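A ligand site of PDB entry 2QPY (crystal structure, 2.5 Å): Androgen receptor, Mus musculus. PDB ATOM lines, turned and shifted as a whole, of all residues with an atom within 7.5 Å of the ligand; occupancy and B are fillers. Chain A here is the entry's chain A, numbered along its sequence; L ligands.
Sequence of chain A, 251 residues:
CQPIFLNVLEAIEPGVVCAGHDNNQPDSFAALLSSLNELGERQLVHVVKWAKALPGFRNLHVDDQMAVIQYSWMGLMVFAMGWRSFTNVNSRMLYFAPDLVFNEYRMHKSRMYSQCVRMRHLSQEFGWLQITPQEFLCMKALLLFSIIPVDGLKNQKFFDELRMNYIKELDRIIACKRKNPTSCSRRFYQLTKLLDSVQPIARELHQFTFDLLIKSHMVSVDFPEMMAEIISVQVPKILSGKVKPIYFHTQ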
ATOM      1  N   PRO A   3      19.009  13.900  24.182  1.00  0.00           N
ATOM      2  CA  PRO A   3      18.523  14.071  25.586  1.00  0.00           C
ATOM      3  C   PRO A   3      17.870  12.790  26.112  1.00  0.00           C
ATOM      4  O   PRO A   3      18.060  12.433  27.267  1.00  0.00           O
ATOM      5  CB  PRO A   3      17.534  15.221  25.571  1.00  0.00           C
ATOM      6  CG  PRO A   3      17.025  15.181  24.130  1.00  0.00           C
ATOM      7  CD  PRO A   3      18.274  14.830  23.287  1.00  0.00           C
ATOM      8  N   ILE A   4      17.107  12.126  25.244  1.00  0.00           N
ATOM      9  CA  ILE A   4      16.426  10.891  25.618  1.00  0.00           C
ATOM     10  C   ILE A   4      17.360   9.689  25.566  1.00  0.00           C
ATOM     11  O   ILE A   4      17.258   8.786  26.397  1.00  0.00           O
ATOM     12  CB  ILE A   4      15.226  10.622  24.683  1.00  0.00           C
ATOM     13  CG1 ILE A   4      14.089  11.595  24.996  1.00  0.00           C
ATOM     14  CG2 ILE A   4      14.750   9.190  24.823  1.00  0.00           C
ATOM     15  CD1 ILE A   4      13.622  11.568  26.451  1.00  0.00           C
ATOM     16  N   PHE A   5      18.260   9.689  24.604  1.00  0.00           N
ATOM     17  CA  PHE A   5      19.212   8.594  24.427  1.00  0.00           C
ATOM     18  C   PHE A   5      20.016   8.333  25.701  1.00  0.00           C
ATOM     19  O   PHE A   5      20.103   7.192  26.178  1.00  0.00           O
ATOM     20  CB  PHE A   5      20.183   8.900  23.282  1.00  0.00           C
ATOM     21  CG  PHE A   5      21.160   7.792  23.010  1.00  0.00           C
ATOM     22  CD1 PHE A   5      20.757   6.634  22.357  1.00  0.00           C
ATOM     23  CD2 PHE A   5      22.488   7.910  23.414  1.00  0.00           C
ATOM     24  CE1 PHE A   5      21.654   5.608  22.114  1.00  0.00           C
ATOM     25  CE2 PHE A   5      23.398   6.879  23.175  1.00  0.00           C
ATOM     26  CZ  PHE A   5      22.983   5.717  22.528  1.00  0.00           C
ATOM     27  N   LEU A   6      20.609   9.385  26.252  1.00  0.00           N
ATOM     28  CA  LEU A   6      21.417   9.276  27.446  1.00  0.00           C
ATOM     29  C   LEU A   6      20.629   8.724  28.639  1.00  0.00           C
ATOM     30  O   LEU A   6      21.194   8.047  29.503  1.00  0.00           O
ATOM     31  CB  LEU A   6      22.026  10.631  27.787  1.00  0.00           C
ATOM     32  CG  LEU A   6      23.391  10.610  28.478  1.00  0.00           C
ATOM     33  CD1 LEU A   6      24.322   9.654  27.742  1.00  0.00           C
ATOM     34  CD2 LEU A   6      23.973  12.019  28.495  1.00  0.00           C
ATOM     35  N   LEU A  54      19.217  -2.190  24.583  1.00  0.00           N
ATOM     36  CA  LEU A  54      19.833  -1.189  23.743  1.00  0.00           C
ATOM     37  C   LEU A  54      18.918  -0.832  22.584  1.00  0.00           C
ATOM     38  O   LEU A  54      18.439  -1.695  21.852  1.00  0.00           O
ATOM     39  CB  LEU A  54      21.173  -1.679  23.192  1.00  0.00           C
ATOM     40  CG  LEU A  54      22.429  -1.137  23.903  1.00  0.00           C
ATOM     41  CD1 LEU A  54      23.673  -1.562  23.136  1.00  0.00           C
ATOM     42  CD2 LEU A  54      22.341   0.385  23.955  1.00  0.00           C
ATOM     43  N   PRO A  55      18.687   0.475  22.385  1.00  0.00           N
ATOM     44  CA  PRO A  55      17.825   0.973  21.302  1.00  0.00           C
ATOM     45  C   PRO A  55      18.325   0.592  19.929  1.00  0.00           C
ATOM     46  O   PRO A  55      19.447   0.900  19.571  1.00  0.00           O
ATOM     47  CB  PRO A  55      17.825   2.483  21.533  1.00  0.00           C
ATOM     48  CG  PRO A  55      19.151   2.730  22.145  1.00  0.00           C
ATOM     49  CD  PRO A  55      19.282   1.598  23.135  1.00  0.00           C
ATOM     50  N   GLY A  56      17.476  -0.086  19.164  1.00  0.00           N
ATOM     51  CA  GLY A  56      17.842  -0.496  17.804  1.00  0.00           C
ATOM     52  C   GLY A  56      18.382  -1.915  17.743  1.00  0.00           C
ATOM     53  O   GLY A  56      18.346  -2.550  16.686  1.00  0.00           O
ATOM     54  N   PHE A  57      18.904  -2.394  18.877  1.00  0.00           N
ATOM     55  CA  PHE A  57      19.477  -3.734  18.932  1.00  0.00           C
ATOM     56  C   PHE A  57      18.446  -4.808  18.539  1.00  0.00           C
ATOM     57  O   PHE A  57      18.786  -5.799  17.884  1.00  0.00           O
ATOM     58  CB  PHE A  57      19.993  -4.028  20.349  1.00  0.00           C
ATOM     59  CG  PHE A  57      20.853  -5.256  20.428  1.00  0.00           C
ATOM     60  CD1 PHE A  57      22.168  -5.208  19.974  1.00  0.00           C
ATOM     61  CD2 PHE A  57      20.344  -6.449  20.928  1.00  0.00           C
ATOM     62  CE1 PHE A  57      22.973  -6.359  20.044  1.00  0.00           C
ATOM     63  CE2 PHE A  57      21.149  -7.601  20.998  1.00  0.00           C
ATOM     64  CZ  PHE A  57      22.468  -7.543  20.543  1.00  0.00           C
ATOM     65  N   ARG A  58      17.200  -4.577  18.935  1.00  0.00           N
ATOM     66  CA  ARG A  58      16.118  -5.527  18.650  1.00  0.00           C
ATOM     67  C   ARG A  58      15.819  -5.642  17.156  1.00  0.00           C
ATOM     68  O   ARG A  58      15.445  -6.709  16.690  1.00  0.00           O
ATOM     69  CB  ARG A  58      14.853  -5.106  19.406  1.00  0.00           C
ATOM     70  CG  ARG A  58      14.215  -6.225  20.202  1.00  0.00           C
ATOM     71  CD  ARG A  58      15.187  -6.801  21.217  1.00  0.00           C
ATOM     72  NE  ARG A  58      14.662  -7.969  21.924  1.00  0.00           N
ATOM     73  CZ  ARG A  58      14.087  -7.931  23.123  1.00  0.00           C
ATOM     74  NH1 ARG A  58      13.967  -6.769  23.788  1.00  0.00           N
ATOM     75  NH2 ARG A  58      13.644  -9.044  23.686  1.00  0.00           N
ATOM     76  N   ASN A  59      15.995  -4.549  16.417  1.00  0.00           N
ATOM     77  CA  ASN A  59      15.740  -4.553  14.989  1.00  0.00           C
ATOM     78  C   ASN A  59      16.932  -5.099  14.216  1.00  0.00           C
ATOM     79  O   ASN A  59      17.136  -4.788  13.058  1.00  0.00           O
ATOM     80  CB  ASN A  59      15.405  -3.158  14.478  1.00  0.00           C
ATOM     81  CG  ASN A  59      13.959  -2.789  14.698  1.00  0.00           C
ATOM     82  OD1 ASN A  59      13.509  -2.593  15.844  1.00  0.00           O
ATOM     83  ND2 ASN A  59      13.195  -2.720  13.590  1.00  0.00           N
ATOM     84  N   LEU A  60      17.730  -5.922  14.893  1.00  0.00           N
ATOM     85  CA  LEU A  60      18.911  -6.529  14.280  1.00  0.00           C
ATOM     86  C   LEU A  60      18.633  -8.011  14.113  1.00  0.00           C
ATOM     87  O   LEU A  60      18.017  -8.628  14.966  1.00  0.00           O
ATOM     88  CB  LEU A  60      20.138  -6.320  15.183  1.00  0.00           C
ATOM     89  CG  LEU A  60      21.384  -5.735  14.520  1.00  0.00           C
ATOM     90  CD1 LEU A  60      22.470  -5.535  15.556  1.00  0.00           C
ATOM     91  CD2 LEU A  60      21.851  -6.667  13.411  1.00  0.00           C
ATOM     92  N   PHE A 145      29.144  -2.700  18.841  1.00  0.00           N
ATOM     93  CA  PHE A 145      29.167  -2.736  17.395  1.00  0.00           C
ATOM     94  C   PHE A 145      30.568  -2.381  16.889  1.00  0.00           C
ATOM     95  O   PHE A 145      30.713  -1.638  15.905  1.00  0.00           O
ATOM     96  CB  PHE A 145      28.162  -1.732  16.837  1.00  0.00           C
ATOM     97  CG  PHE A 145      26.878  -1.663  17.605  1.00  0.00           C
ATOM     98  CD1 PHE A 145      25.853  -2.576  17.362  1.00  0.00           C
ATOM     99  CD2 PHE A 145      26.690  -0.693  18.576  1.00  0.00           C
ATOM    100  CE1 PHE A 145      24.668  -2.521  18.096  1.00  0.00           C
ATOM    101  CE2 PHE A 145      25.514  -0.619  19.308  1.00  0.00           C
ATOM    102  CZ  PHE A 145      24.493  -1.533  19.073  1.00  0.00           C
ATOM    103  N   PHE A 158      21.588  -2.984   8.175  1.00  0.00           N
ATOM    104  CA  PHE A 158      21.057  -2.414   9.400  1.00  0.00           C
ATOM    105  C   PHE A 158      22.135  -2.143  10.447  1.00  0.00           C
ATOM    106  O   PHE A 158      22.025  -1.180  11.214  1.00  0.00           O
ATOM    107  CB  PHE A 158      19.970  -3.340   9.979  1.00  0.00           C
ATOM    108  CG  PHE A 158      18.909  -2.621  10.741  1.00  0.00           C
ATOM    109  CD1 PHE A 158      19.192  -1.990  11.960  1.00  0.00           C
ATOM    110  CD2 PHE A 158      17.612  -2.546  10.247  1.00  0.00           C
ATOM    111  CE1 PHE A 158      18.214  -1.302  12.675  1.00  0.00           C
ATOM    112  CE2 PHE A 158      16.609  -1.871  10.951  1.00  0.00           C
ATOM    113  CZ  PHE A 158      16.912  -1.249  12.169  1.00  0.00           C
ATOM    114  N   GLU A 161      23.964   1.110   9.882  1.00  0.00           N
ATOM    115  CA  GLU A 161      23.034   2.202  10.184  1.00  0.00           C
ATOM    116  C   GLU A 161      22.996   2.470  11.683  1.00  0.00           C
ATOM    117  O   GLU A 161      23.063   3.610  12.129  1.00  0.00           O
ATOM    118  CB  GLU A 161      21.635   1.846   9.671  1.00  0.00           C
ATOM    119  CG  GLU A 161      20.791   3.035   9.203  1.00  0.00           C
ATOM    120  CD  GLU A 161      20.132   3.779  10.342  1.00  0.00           C
ATOM    121  OE1 GLU A 161      19.344   3.144  11.093  1.00  0.00           O
ATOM    122  OE2 GLU A 161      20.379   5.008  10.481  1.00  0.00           O
ATOM    123  N   LEU A 162      22.896   1.406  12.463  1.00  0.00           N
ATOM    124  CA  LEU A 162      22.873   1.519  13.905  1.00  0.00           C
ATOM    125  C   LEU A 162      24.204   2.080  14.429  1.00  0.00           C
ATOM    126  O   LEU A 162      24.211   3.019  15.221  1.00  0.00           O
ATOM    127  CB  LEU A 162      22.597   0.145  14.524  1.00  0.00           C
ATOM    128  CG  LEU A 162      21.914   0.143  15.894  1.00  0.00           C
ATOM    129  CD1 LEU A 162      20.728   1.115  15.890  1.00  0.00           C
ATOM    130  CD2 LEU A 162      21.437  -1.272  16.231  1.00  0.00           C
ATOM    131  N   ARG A 163      25.313   1.496  13.996  1.00  0.00           N
ATOM    132  CA  ARG A 163      26.620   1.929  14.395  1.00  0.00           C
ATOM    133  C   ARG A 163      26.765   3.417  14.121  1.00  0.00           C
ATOM    134  O   ARG A 163      27.274   4.171  14.953  1.00  0.00           O
ATOM    135  CB  ARG A 163      27.696   1.158  13.619  1.00  0.00           C
ATOM    136  CG  ARG A 163      29.126   1.628  13.873  1.00  0.00           C
ATOM    137  CD  ARG A 163      30.145   0.701  13.218  1.00  0.00           C
ATOM    138  NE  ARG A 163      31.486   1.253  13.232  1.00  0.00           N
ATOM    139  CZ  ARG A 163      32.239   1.402  14.308  1.00  0.00           C
ATOM    140  NH1 ARG A 163      31.781   1.028  15.498  1.00  0.00           N
ATOM    141  NH2 ARG A 163      33.461   1.923  14.213  1.00  0.00           N
ATOM    142  N   MET A 164      26.311   3.840  12.956  1.00  0.00           N
ATOM    143  CA  MET A 164      26.361   5.228  12.542  1.00  0.00           C
ATOM    144  C   MET A 164      25.619   6.129  13.535  1.00  0.00           C
ATOM    145  O   MET A 164      26.066   7.221  13.849  1.00  0.00           O
ATOM    146  CB  MET A 164      25.758   5.376  11.147  1.00  0.00           C
ATOM    147  CG  MET A 164      25.534   6.833  10.706  1.00  0.00           C
ATOM    148  SD  MET A 164      24.941   6.934   9.004  1.00  0.00           S
ATOM    149  CE  MET A 164      23.216   6.479   9.221  1.00  0.00           C
ATOM    150  N   ASN A 165      24.480   5.649  14.013  1.00  0.00           N
ATOM    151  CA  ASN A 165      23.671   6.409  14.972  1.00  0.00           C
ATOM    152  C   ASN A 165      24.344   6.531  16.319  1.00  0.00           C
ATOM    153  O   ASN A 165      24.293   7.583  16.959  1.00  0.00           O
ATOM    154  CB  ASN A 165      22.300   5.773  15.127  1.00  0.00           C
ATOM    155  CG  ASN A 165      21.302   6.245  14.071  1.00  0.00           C
ATOM    156  OD1 ASN A 165      20.996   7.437  13.994  1.00  0.00           O
ATOM    157  ND2 ASN A 165      20.805   5.313  13.261  1.00  0.00           N
ATOM    158  N   TYR A 166      24.985   5.458  16.773  1.00  0.00           N
ATOM    159  CA  TYR A 166      25.687   5.493  18.050  1.00  0.00           C
ATOM    160  C   TYR A 166      26.933   6.377  17.964  1.00  0.00           C
ATOM    161  O   TYR A 166      27.314   7.028  18.925  1.00  0.00           O
ATOM    162  CB  TYR A 166      26.075   4.090  18.509  1.00  0.00           C
ATOM    163  CG  TYR A 166      24.939   3.321  19.129  1.00  0.00           C
ATOM    164  CD1 TYR A 166      24.007   2.644  18.353  1.00  0.00           C
ATOM    165  CD2 TYR A 166      24.782   3.286  20.516  1.00  0.00           C
ATOM    166  CE1 TYR A 166      22.941   1.961  18.932  1.00  0.00           C
ATOM    167  CE2 TYR A 166      23.712   2.606  21.109  1.00  0.00           C
ATOM    168  CZ  TYR A 166      22.803   1.948  20.311  1.00  0.00           C
ATOM    169  OH  TYR A 166      21.745   1.273  20.897  1.00  0.00           O
ATOM    170  N   LYS A 168      27.080   8.921  16.242  1.00  0.00           N
ATOM    171  CA  LYS A 168      26.516  10.265  16.241  1.00  0.00           C
ATOM    172  C   LYS A 168      26.097  10.638  17.649  1.00  0.00           C
ATOM    173  O   LYS A 168      26.180  11.796  18.042  1.00  0.00           O
ATOM    174  CB  LYS A 168      25.303  10.341  15.311  1.00  0.00           C
ATOM    175  CG  LYS A 168      24.530  11.644  15.398  1.00  0.00           C
ATOM    176  CD  LYS A 168      23.393  11.688  14.389  1.00  0.00           C
ATOM    177  CE  LYS A 168      22.681  13.036  14.434  1.00  0.00           C
ATOM    178  NZ  LYS A 168      21.687  13.158  13.320  1.00  0.00           N
ATOM    179  N   GLU A 169      25.651   9.653  18.420  1.00  0.00           N
ATOM    180  CA  GLU A 169      25.244   9.886  19.798  1.00  0.00           C
ATOM    181  C   GLU A 169      26.439  10.298  20.645  1.00  0.00           C
ATOM    182  O   GLU A 169      26.332  11.134  21.525  1.00  0.00           O
ATOM    183  CB  GLU A 169      24.618   8.615  20.401  1.00  0.00           C
ATOM    184  CG  GLU A 169      23.137   8.452  20.077  1.00  0.00           C
ATOM    185  CD  GLU A 169      22.335   9.693  20.425  1.00  0.00           C
ATOM    186  OE1 GLU A 169      22.545  10.252  21.540  1.00  0.00           O
ATOM    187  OE2 GLU A 169      21.491  10.112  19.611  1.00  0.00           O
ATOM    188  N   ARG A 172      27.162  13.847  19.868  1.00  0.00           N
ATOM    189  CA  ARG A 172      26.184  14.712  20.518  1.00  0.00           C
ATOM    190  C   ARG A 172      26.542  14.941  21.990  1.00  0.00           C
ATOM    191  O   ARG A 172      26.554  16.073  22.455  1.00  0.00           O
ATOM    192  CB  ARG A 172      24.780  14.097  20.407  1.00  0.00           C
ATOM    193  CG  ARG A 172      24.292  13.994  18.972  1.00  0.00           C
ATOM    194  CD  ARG A 172      23.410  12.763  18.770  1.00  0.00           C
ATOM    195  NE  ARG A 172      22.040  12.949  19.252  1.00  0.00           N
ATOM    196  CZ  ARG A 172      21.169  13.787  18.697  1.00  0.00           C
ATOM    197  NH1 ARG A 172      21.518  14.521  17.635  1.00  0.00           N
ATOM    198  NH2 ARG A 172      19.934  13.887  19.200  1.00  0.00           N
HETATM  199  C1  LIG L   1      17.701   8.009  18.313  1.00  0.00           C
HETATM  200  C2  LIG L   1      17.788   3.579  15.465  1.00  0.00           C
HETATM  201  C3  LIG L   1      17.072   7.884  16.999  1.00  0.00           C
HETATM  202  C4  LIG L   1      16.877   3.132  16.403  1.00  0.00           C
HETATM  203  C5  LIG L   1      17.373   6.768  16.193  1.00  0.00           C
HETATM  204  C6  LIG L   1      15.994   2.110  16.129  1.00  0.00           C
HETATM  205  C7  LIG L   1      18.311   5.793  16.595  1.00  0.00           C
HETATM  206  C8  LIG L   1      16.013   1.484  14.837  1.00  0.00           C
HETATM  207  C9  LIG L   1      18.923   5.933  17.887  1.00  0.00           C
HETATM  208  C10 LIG L   1      16.937   1.931  13.857  1.00  0.00           C
HETATM  209  C11 LIG L   1      18.612   7.080  18.735  1.00  0.00           C
HETATM  210  C12 LIG L   1      17.839   2.995  14.170  1.00  0.00           C
HETATM  211  C13 LIG L   1      17.352   9.166  19.195  1.00  0.00           C
HETATM  212  C14 LIG L   1      17.840  10.562  18.679  1.00  0.00           C
HETATM  213  I1  LIG L   1      16.414   6.596  14.323  1.00  0.00           I
HETATM  214  I2  LIG L   1      14.650   1.520  17.635  1.00  0.00           I
HETATM  215  I3  LIG L   1      20.437   4.550  18.450  1.00  0.00           I
HETATM  216  O1  LIG L   1      18.829  11.069  19.271  1.00  0.00           O
HETATM  217  O2  LIG L   1      18.653   4.643  15.821  1.00  0.00           O
HETATM  218  O3  LIG L   1      15.114   0.448  14.570  1.00  0.00           O
HETATM  219  O4  LIG L   1      17.200  11.082  17.717  1.00  0.00           O
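The side-chain carboxylate (OE2) of Glu 161 lies within hydrogen-bond range of the side-chain amide nitrogen (ND2) of Asn 165, at 2.8 Å.
O of Pro 55 is in hydrogen-bond range of OH of Tyr 166, 2.7 Å away.
OE2 of Glu 169 is in salt-bridge range of NE of Arg 172 (2.9 Å).
Pro 55 touches the ligand.
Gly 56 touches the ligand (N to I2, 3.6 Å).
CG of Asn 59 touches O3 of the ligand, at 3.4 Å.
Phe 158 touches the ligand (CZ to O3, 3.4 Å).
Glu 161 touches the ligand (OE1 to C12, 3.4 Å).
CD1 of Leu 162 touches C12 of the ligand, 3.9 Å away.
Tyr 166 touches the ligand.
Hydrophobic or aromatic side chains within 4 Å of the ligand: Phe 158, Leu 162 and Tyr 166.
Of the 22 residues printed, 10 come within 4 Å of the ligand.
The nearest printed residue that does not touch the ligand is Phe 5 (4.003 Å).
An oxygen (O2) of the ligand lies within hydrogen-bond range of the side-chain amide nitrogen of Asn 165.
An oxygen (O1) of the ligand is in salt-bridge range of the guanidinium group (NH2) of Arg 172 (3.0 Å).
OE2 of Glu 169 sits close to O1 of the ligand, 2.8 Å away.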
